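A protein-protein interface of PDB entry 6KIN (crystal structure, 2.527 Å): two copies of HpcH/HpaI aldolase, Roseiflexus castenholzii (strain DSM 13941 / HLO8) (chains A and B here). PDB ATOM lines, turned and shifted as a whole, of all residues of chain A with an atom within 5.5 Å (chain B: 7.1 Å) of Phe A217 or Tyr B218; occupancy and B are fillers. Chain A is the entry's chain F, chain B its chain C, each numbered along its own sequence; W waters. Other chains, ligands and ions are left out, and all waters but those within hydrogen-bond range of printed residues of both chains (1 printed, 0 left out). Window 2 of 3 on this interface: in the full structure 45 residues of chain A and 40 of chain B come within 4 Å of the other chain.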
ATOM      1  N   PRO A 200      24.589  26.542  -8.078  1.00  0.00           N
ATOM      2  CA  PRO A 200      24.445  26.712  -9.538  1.00  0.00           C
ATOM      3  C   PRO A 200      25.103  25.623 -10.350  1.00  0.00           C
ATOM      4  O   PRO A 200      24.789  25.483 -11.538  1.00  0.00           O
ATOM      5  CB  PRO A 200      25.112  28.068  -9.798  1.00  0.00           C
ATOM      6  CG  PRO A 200      26.114  28.193  -8.717  1.00  0.00           C
ATOM      7  CD  PRO A 200      25.465  27.576  -7.497  1.00  0.00           C
ATOM      8  N   PHE A 201      26.002  24.845  -9.757  1.00  0.00           N
ATOM      9  CA  PHE A 201      26.767  23.856 -10.494  1.00  0.00           C
ATOM     10  C   PHE A 201      26.154  22.469 -10.415  1.00  0.00           C
ATOM     11  O   PHE A 201      26.781  21.504 -10.857  1.00  0.00           O
ATOM     12  CB  PHE A 201      28.213  23.831  -9.998  1.00  0.00           C
ATOM     13  CG  PHE A 201      28.988  25.096 -10.298  1.00  0.00           C
ATOM     14  CD1 PHE A 201      28.540  26.006 -11.255  1.00  0.00           C
ATOM     15  CD2 PHE A 201      30.184  25.365  -9.628  1.00  0.00           C
ATOM     16  CE1 PHE A 201      29.270  27.167 -11.536  1.00  0.00           C
ATOM     17  CE2 PHE A 201      30.915  26.517  -9.901  1.00  0.00           C
ATOM     18  CZ  PHE A 201      30.459  27.417 -10.857  1.00  0.00           C
ATOM     19  N   TYR A 202      24.948  22.341  -9.863  1.00  0.00           N
ATOM     20  CA  TYR A 202      24.211  21.079  -9.921  1.00  0.00           C
ATOM     21  C   TYR A 202      23.339  21.106 -11.180  1.00  0.00           C
ATOM     22  O   TYR A 202      22.299  21.765 -11.227  1.00  0.00           O
ATOM     23  CB  TYR A 202      23.393  20.861  -8.649  1.00  0.00           C
ATOM     24  CG  TYR A 202      22.639  19.546  -8.660  1.00  0.00           C
ATOM     25  CD1 TYR A 202      23.266  18.376  -9.063  1.00  0.00           C
ATOM     26  CD2 TYR A 202      21.302  19.479  -8.300  1.00  0.00           C
ATOM     27  CE1 TYR A 202      22.593  17.178  -9.100  1.00  0.00           C
ATOM     28  CE2 TYR A 202      20.616  18.286  -8.326  1.00  0.00           C
ATOM     29  CZ  TYR A 202      21.268  17.140  -8.726  1.00  0.00           C
ATOM     30  OH  TYR A 202      20.602  15.943  -8.770  1.00  0.00           O
ATOM     31  N   GLY A 203      23.772  20.407 -12.218  1.00  0.00           N
ATOM     32  CA  GLY A 203      22.990  20.384 -13.437  1.00  0.00           C
ATOM     33  C   GLY A 203      23.527  19.305 -14.341  1.00  0.00           C
ATOM     34  O   GLY A 203      24.503  18.621 -14.016  1.00  0.00           O
ATOM     35  N   VAL A 204      22.874  19.146 -15.484  1.00  0.00           N
ATOM     36  CA  VAL A 204      23.295  18.161 -16.476  1.00  0.00           C
ATOM     37  C   VAL A 204      23.763  18.878 -17.740  1.00  0.00           C
ATOM     38  O   VAL A 204      23.185  19.889 -18.154  1.00  0.00           O
ATOM     39  CB  VAL A 204      22.172  17.150 -16.786  1.00  0.00           C
ATOM     40  CG1 VAL A 204      21.960  16.228 -15.598  1.00  0.00           C
ATOM     41  CG2 VAL A 204      20.890  17.867 -17.123  1.00  0.00           C
ATOM     42  N   LEU A 205      24.823  18.344 -18.346  1.00  0.00           N
ATOM     43  CA  LEU A 205      25.436  18.907 -19.546  1.00  0.00           C
ATOM     44  C   LEU A 205      24.797  18.282 -20.782  1.00  0.00           C
ATOM     45  O   LEU A 205      24.589  17.065 -20.829  1.00  0.00           O
ATOM     46  CB  LEU A 205      26.950  18.646 -19.532  1.00  0.00           C
ATOM     47  CG  LEU A 205      27.969  19.570 -20.220  1.00  0.00           C
ATOM     48  CD1 LEU A 205      27.969  20.932 -19.576  1.00  0.00           C
ATOM     49  CD2 LEU A 205      29.365  18.981 -20.168  1.00  0.00           C
ATOM     50  N   ALA A 206      24.474  19.110 -21.769  1.00  0.00           N
ATOM     51  CA  ALA A 206      23.934  18.581 -23.014  1.00  0.00           C
ATOM     52  C   ALA A 206      24.992  17.750 -23.747  1.00  0.00           C
ATOM     53  O   ALA A 206      26.178  17.757 -23.404  1.00  0.00           O
ATOM     54  CB  ALA A 206      23.448  19.708 -23.918  1.00  0.00           C
ATOM     55  N   ARG A 215      27.934  24.477 -25.205  1.00  0.00           N
ATOM     56  CA  ARG A 215      27.284  23.256 -24.713  1.00  0.00           C
ATOM     57  C   ARG A 215      26.349  23.577 -23.555  1.00  0.00           C
ATOM     58  O   ARG A 215      26.830  23.809 -22.433  1.00  0.00           O
ATOM     59  CB  ARG A 215      28.342  22.246 -24.260  1.00  0.00           C
ATOM     60  CG  ARG A 215      28.121  20.840 -24.727  1.00  0.00           C
ATOM     61  CD  ARG A 215      29.246  19.952 -24.231  1.00  0.00           C
ATOM     62  NE  ARG A 215      28.765  18.626 -23.853  1.00  0.00           N
ATOM     63  CZ  ARG A 215      29.564  17.610 -23.563  1.00  0.00           C
ATOM     64  NH1 ARG A 215      30.879  17.777 -23.604  1.00  0.00           N
ATOM     65  NH2 ARG A 215      29.058  16.427 -23.238  1.00  0.00           N
ATOM     66  N   PRO A 216      25.035  23.582 -23.757  1.00  0.00           N
ATOM     67  CA  PRO A 216      24.116  24.036 -22.702  1.00  0.00           C
ATOM     68  C   PRO A 216      24.164  23.193 -21.426  1.00  0.00           C
ATOM     69  O   PRO A 216      24.571  22.026 -21.406  1.00  0.00           O
ATOM     70  CB  PRO A 216      22.735  23.952 -23.374  1.00  0.00           C
ATOM     71  CG  PRO A 216      22.940  23.182 -24.630  1.00  0.00           C
ATOM     72  CD  PRO A 216      24.348  23.400 -25.042  1.00  0.00           C
ATOM     73  N   PHE A 217      23.725  23.816 -20.337  1.00  0.00           N
ATOM     74  CA  PHE A 217      23.844  23.254 -18.994  1.00  0.00           C
ATOM     75  C   PHE A 217      22.535  23.523 -18.265  1.00  0.00           C
ATOM     76  O   PHE A 217      22.197  24.684 -18.009  1.00  0.00           O
ATOM     77  CB  PHE A 217      25.039  23.878 -18.268  1.00  0.00           C
ATOM     78  CG  PHE A 217      25.254  23.382 -16.861  1.00  0.00           C
ATOM     79  CD1 PHE A 217      25.834  22.142 -16.627  1.00  0.00           C
ATOM     80  CD2 PHE A 217      24.919  24.178 -15.777  1.00  0.00           C
ATOM     81  CE1 PHE A 217      26.064  21.698 -15.335  1.00  0.00           C
ATOM     82  CE2 PHE A 217      25.136  23.743 -14.483  1.00  0.00           C
ATOM     83  CZ  PHE A 217      25.713  22.500 -14.257  1.00  0.00           C
ATOM     84  N   TYR A 218      21.795  22.463 -17.937  1.00  0.00           N
ATOM     85  CA  TYR A 218      20.467  22.578 -17.331  1.00  0.00           C
ATOM     86  C   TYR A 218      20.566  22.327 -15.826  1.00  0.00           C
ATOM     87  O   TYR A 218      20.840  21.201 -15.394  1.00  0.00           O
ATOM     88  CB  TYR A 218      19.497  21.598 -17.979  1.00  0.00           C
ATOM     89  CG  TYR A 218      19.408  21.680 -19.491  1.00  0.00           C
ATOM     90  CD1 TYR A 218      18.404  22.436 -20.110  1.00  0.00           C
ATOM     91  CD2 TYR A 218      20.306  20.973 -20.311  1.00  0.00           C
ATOM     92  CE1 TYR A 218      18.303  22.502 -21.500  1.00  0.00           C
ATOM     93  CE2 TYR A 218      20.203  21.026 -21.713  1.00  0.00           C
ATOM     94  CZ  TYR A 218      19.201  21.794 -22.291  1.00  0.00           C
ATOM     95  OH  TYR A 218      19.095  21.860 -23.658  1.00  0.00           O
ATOM     96  N   GLN A 219      20.326  23.368 -15.035  1.00  0.00           N
ATOM     97  CA  GLN A 219      20.437  23.256 -13.587  1.00  0.00           C
ATOM     98  C   GLN A 219      19.336  22.355 -13.014  1.00  0.00           C
ATOM     99  O   GLN A 219      18.230  22.255 -13.553  1.00  0.00           O
ATOM    100  CB  GLN A 219      20.376  24.645 -12.936  1.00  0.00           C
ATOM    101  CG  GLN A 219      21.675  25.452 -13.029  1.00  0.00           C
ATOM    102  CD  GLN A 219      21.594  26.830 -12.363  1.00  0.00           C
ATOM    103  OE1 GLN A 219      21.114  26.971 -11.236  1.00  0.00           O
ATOM    104  NE2 GLN A 219      22.073  27.853 -13.070  1.00  0.00           N
ATOM    105  N   TYR B 202       7.254  25.100 -10.943  1.00  0.00           N
ATOM    106  CA  TYR B 202       8.225  24.197 -10.324  1.00  0.00           C
ATOM    107  C   TYR B 202       9.550  24.265 -11.100  1.00  0.00           C
ATOM    108  O   TYR B 202       9.730  23.582 -12.111  1.00  0.00           O
ATOM    109  CB  TYR B 202       7.680  22.768 -10.244  1.00  0.00           C
ATOM    110  CG  TYR B 202       8.564  21.843  -9.411  1.00  0.00           C
ATOM    111  CD1 TYR B 202       8.923  22.197  -8.113  1.00  0.00           C
ATOM    112  CD2 TYR B 202       9.058  20.637  -9.925  1.00  0.00           C
ATOM    113  CE1 TYR B 202       9.736  21.393  -7.344  1.00  0.00           C
ATOM    114  CE2 TYR B 202       9.879  19.810  -9.148  1.00  0.00           C
ATOM    115  CZ  TYR B 202      10.212  20.202  -7.854  1.00  0.00           C
ATOM    116  OH  TYR B 202      11.032  19.446  -7.037  1.00  0.00           O
ATOM    117  N   GLY B 203      10.496  25.068 -10.609  1.00  0.00           N
ATOM    118  CA  GLY B 203      11.758  25.209 -11.308  1.00  0.00           C
ATOM    119  C   GLY B 203      12.866  25.710 -10.410  1.00  0.00           C
ATOM    120  O   GLY B 203      12.663  26.005  -9.233  1.00  0.00           O
ATOM    121  N   VAL B 204      14.061  25.800 -10.978  1.00  0.00           N
ATOM    122  CA  VAL B 204      15.223  26.353 -10.290  1.00  0.00           C
ATOM    123  C   VAL B 204      15.535  27.716 -10.899  1.00  0.00           C
ATOM    124  O   VAL B 204      15.599  27.856 -12.127  1.00  0.00           O
ATOM    125  CB  VAL B 204      16.436  25.407 -10.369  1.00  0.00           C
ATOM    126  CG1 VAL B 204      17.642  26.018  -9.674  1.00  0.00           C
ATOM    127  CG2 VAL B 204      16.099  24.094  -9.710  1.00  0.00           C
ATOM    128  N   LEU B 205      15.698  28.725 -10.045  1.00  0.00           N
ATOM    129  CA  LEU B 205      16.052  30.061 -10.488  1.00  0.00           C
ATOM    130  C   LEU B 205      17.563  30.190 -10.511  1.00  0.00           C
ATOM    131  O   LEU B 205      18.233  29.889  -9.518  1.00  0.00           O
ATOM    132  CB  LEU B 205      15.451  31.128  -9.572  1.00  0.00           C
ATOM    133  CG  LEU B 205      15.526  32.535 -10.161  1.00  0.00           C
ATOM    134  CD1 LEU B 205      14.574  32.653 -11.327  1.00  0.00           C
ATOM    135  CD2 LEU B 205      15.213  33.594  -9.117  1.00  0.00           C
ATOM    136  N   ALA B 206      18.095  30.626 -11.648  1.00  0.00           N
ATOM    137  CA  ALA B 206      19.527  30.823 -11.785  1.00  0.00           C
ATOM    138  C   ALA B 206      20.002  31.979 -10.903  1.00  0.00           C
ATOM    139  O   ALA B 206      19.228  32.852 -10.493  1.00  0.00           O
ATOM    140  CB  ALA B 206      19.891  31.086 -13.248  1.00  0.00           C
ATOM    141  N   ASP B 207      21.301  31.970 -10.627  1.00  0.00           N
ATOM    142  CA  ASP B 207      21.909  33.070  -9.847  1.00  0.00           C
ATOM    143  C   ASP B 207      21.949  34.317 -10.733  1.00  0.00           C
ATOM    144  O   ASP B 207      21.963  34.199 -11.961  1.00  0.00           O
ATOM    145  CB  ASP B 207      23.309  32.712  -9.351  1.00  0.00           C
ATOM    146  CG  ASP B 207      23.361  31.666  -8.254  1.00  0.00           C
ATOM    147  OD1 ASP B 207      22.307  31.337  -7.714  1.00  0.00           O
ATOM    148  OD2 ASP B 207      24.462  31.203  -7.944  1.00  0.00           O
ATOM    149  N   ARG B 215      17.022  36.356 -15.273  1.00  0.00           N
ATOM    150  CA  ARG B 215      17.677  35.197 -14.627  1.00  0.00           C
ATOM    151  C   ARG B 215      16.940  33.988 -15.188  1.00  0.00           C
ATOM    152  O   ARG B 215      15.741  33.898 -14.991  1.00  0.00           O
ATOM    153  CB  ARG B 215      17.472  35.210 -13.117  1.00  0.00           C
ATOM    154  CG  ARG B 215      18.214  36.312 -12.395  1.00  0.00           C
ATOM    155  CD  ARG B 215      17.728  36.346 -10.971  1.00  0.00           C
ATOM    156  NE  ARG B 215      18.450  35.434 -10.112  1.00  0.00           N
ATOM    157  CZ  ARG B 215      18.384  35.464  -8.803  1.00  0.00           C
ATOM    158  NH1 ARG B 215      17.720  36.427  -8.206  1.00  0.00           N
ATOM    159  NH2 ARG B 215      18.976  34.535  -8.093  1.00  0.00           N
ATOM    160  N   PRO B 216      17.660  33.133 -15.888  1.00  0.00           N
ATOM    161  CA  PRO B 216      17.073  31.935 -16.512  1.00  0.00           C
ATOM    162  C   PRO B 216      16.355  31.040 -15.506  1.00  0.00           C
ATOM    163  O   PRO B 216      16.795  30.862 -14.364  1.00  0.00           O
ATOM    164  CB  PRO B 216      18.291  31.218 -17.113  1.00  0.00           C
ATOM    165  CG  PRO B 216      19.361  32.269 -17.213  1.00  0.00           C
ATOM    166  CD  PRO B 216      19.113  33.238 -16.104  1.00  0.00           C
ATOM    167  N   PHE B 217      15.259  30.444 -15.955  1.00  0.00           N
ATOM    168  CA  PHE B 217      14.418  29.605 -15.113  1.00  0.00           C
ATOM    169  C   PHE B 217      14.346  28.207 -15.713  1.00  0.00           C
ATOM    170  O   PHE B 217      13.967  28.047 -16.881  1.00  0.00           O
ATOM    171  CB  PHE B 217      13.026  30.218 -14.973  1.00  0.00           C
ATOM    172  CG  PHE B 217      12.161  29.513 -13.992  1.00  0.00           C
ATOM    173  CD1 PHE B 217      12.456  29.549 -12.650  1.00  0.00           C
ATOM    174  CD2 PHE B 217      11.055  28.813 -14.412  1.00  0.00           C
ATOM    175  CE1 PHE B 217      11.662  28.916 -11.751  1.00  0.00           C
ATOM    176  CE2 PHE B 217      10.256  28.167 -13.512  1.00  0.00           C
ATOM    177  CZ  PHE B 217      10.558  28.219 -12.181  1.00  0.00           C
ATOM    178  N   TYR B 218      14.722  27.196 -14.926  1.00  0.00           N
ATOM    179  CA  TYR B 218      14.761  25.811 -15.393  1.00  0.00           C
ATOM    180  C   TYR B 218      13.666  25.014 -14.701  1.00  0.00           C
ATOM    181  O   TYR B 218      13.739  24.776 -13.489  1.00  0.00           O
ATOM    182  CB  TYR B 218      16.115  25.160 -15.120  1.00  0.00           C
ATOM    183  CG  TYR B 218      17.340  25.908 -15.597  1.00  0.00           C
ATOM    184  CD1 TYR B 218      17.832  27.007 -14.891  1.00  0.00           C
ATOM    185  CD2 TYR B 218      18.030  25.490 -16.733  1.00  0.00           C
ATOM    186  CE1 TYR B 218      18.966  27.675 -15.313  1.00  0.00           C
ATOM    187  CE2 TYR B 218      19.167  26.150 -17.162  1.00  0.00           C
ATOM    188  CZ  TYR B 218      19.628  27.243 -16.449  1.00  0.00           C
ATOM    189  OH  TYR B 218      20.762  27.900 -16.869  1.00  0.00           O
ATOM    190  N   GLN B 219      12.675  24.568 -15.465  1.00  0.00           N
ATOM    191  CA  GLN B 219      11.616  23.760 -14.873  1.00  0.00           C
ATOM    192  C   GLN B 219      12.138  22.392 -14.457  1.00  0.00           C
ATOM    193  O   GLN B 219      13.044  21.829 -15.083  1.00  0.00           O
ATOM    194  CB  GLN B 219      10.463  23.580 -15.845  1.00  0.00           C
ATOM    195  CG  GLN B 219       9.618  24.790 -16.013  1.00  0.00           C
ATOM    196  CD  GLN B 219       8.449  24.512 -16.907  1.00  0.00           C
ATOM    197  OE1 GLN B 219       7.757  23.493 -16.753  1.00  0.00           O
ATOM    198  NE2 GLN B 219       8.221  25.402 -17.875  1.00  0.00           N
ATOM    199  N   GLN B 220      11.544  21.854 -13.392  1.00  0.00           N
ATOM    200  CA  GLN B 220      11.945  20.575 -12.830  1.00  0.00           C
ATOM    201  C   GLN B 220      10.819  19.551 -12.959  1.00  0.00           C
ATOM    202  O   GLN B 220       9.651  19.901 -13.110  1.00  0.00           O
ATOM    203  CB  GLN B 220      12.367  20.731 -11.365  1.00  0.00           C
ATOM    204  CG  GLN B 220      13.477  21.732 -11.123  1.00  0.00           C
ATOM    205  CD  GLN B 220      14.772  21.378 -11.836  1.00  0.00           C
ATOM    206  OE1 GLN B 220      15.360  20.341 -11.595  1.00  0.00           O
ATOM    207  NE2 GLN B 220      15.220  22.257 -12.719  1.00  0.00           N
ATOM    208  N   ASP B 221      11.193  18.267 -12.914  1.00  0.00           N
ATOM    209  CA  ASP B 221      10.235  17.172 -13.052  1.00  0.00           C
ATOM    210  C   ASP B 221       9.538  16.922 -11.713  1.00  0.00           C
ATOM    211  O   ASP B 221      10.192  16.557 -10.722  1.00  0.00           O
ATOM    212  CB  ASP B 221      10.944  15.914 -13.545  1.00  0.00           C
ATOM    213  CG  ASP B 221      10.037  14.695 -13.597  1.00  0.00           C
ATOM    214  OD1 ASP B 221       8.803  14.848 -13.574  1.00  0.00           O
ATOM    215  OD2 ASP B 221      10.566  13.556 -13.686  1.00  0.00           O
HETATM  216  O   HOH W   1      23.279  28.720 -16.152  1.00  0.00           O
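The backbone carbonyl oxygen (O) of Gln A219 sits at hydrogen-bond distance from the side-chain amide nitrogen (NE2) of Gln B220.
Water W1 bridges the side-chain hydroxyl of Tyr B218 and the side-chain amide nitrogen of Gln A219.
Among the printed residues, merely in contact across the chains: Phe A217 with Tyr B218 (3.5 Å), Pro A200 with Asp B207 (3.5 Å), Gln A219 with Tyr B218 (3.6 Å), Tyr A218 with Tyr B218 (3.8 Å), Gln A219 with Ala B206 (3.9 Å) and Gln A219 with Val B204 (3.9 Å).
Of the 12 printed residues of chain A, 4 touch a printed residue of chain B.
Printed residues of chain A that touch a printed residue of chain B: Pro A200, Phe A217, Tyr A218 and Gln A219.
Among the printed residues, 7 pairs touch across the chains.
Phe A217 touches one residue of chain B.
Of chain A, only Phe A217 (3.5 Å), Tyr A218 (3.8 Å) and Gln A219 (3.6 Å) come within 4 Å of Tyr B218.
Of the printed residues of chain A, Gln B220 touches Gln A219.
Of the printed residues of chain B, Gln A219 touches Val B204 (3.9 Å), Ala B206 (3.9 Å), Tyr B218 (3.6 Å) and Gln B220 (3.1 Å).
The nearest printed residue of chain B that does not touch Phe A217 is Pro B216 (7.7 Å).
The nearest printed residue of chain A that does not touch Tyr B218 is Pro A200 (7.1 Å).
The backbone NH (N) of Val A204 lies within hydrogen-bond range of the backbone carbonyl oxygen (O) of Tyr A218 (2.9 Å).
NE2 of Gln B220 is in hydrogen-bond range of O of Tyr B218.
The backbone NH of Gln B220 sits at hydrogen-bond distance from the backbone carbonyl oxygen of Tyr B202 (2.8 Å).
N of Val B204 sits at hydrogen-bond distance from O of Tyr B218 (2.7 Å).
O of Ala B206 is in hydrogen-bond range of NE of Arg B215, 2.7 Å away.
The backbone NH of Ala B206 lies within hydrogen-bond range of the backbone carbonyl oxygen of Pro B216 (3.0 Å).
Tyr A218 touches its own counterpart, Tyr B218.
Gln A219 touches Val B204, but with the chains exchanged Val A204 does not touch Gln B219 (9.0 Å).
Gln A219 touches Ala B206, but with the chains exchanged Ala A206 does not touch Gln B219 (13.5 Å).
Gln A219 touches Tyr B218, but with the chains exchanged Tyr A218 does not touch Gln B219 (7.1 Å).
Positions printed for both chains: 202, 203, 204, 205, 206, 215, 216, 217, 218 and 219.
Of the 7 pairs that touch across the chains among the printed residues, 1 has its exchanged pair printed and touching as well.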
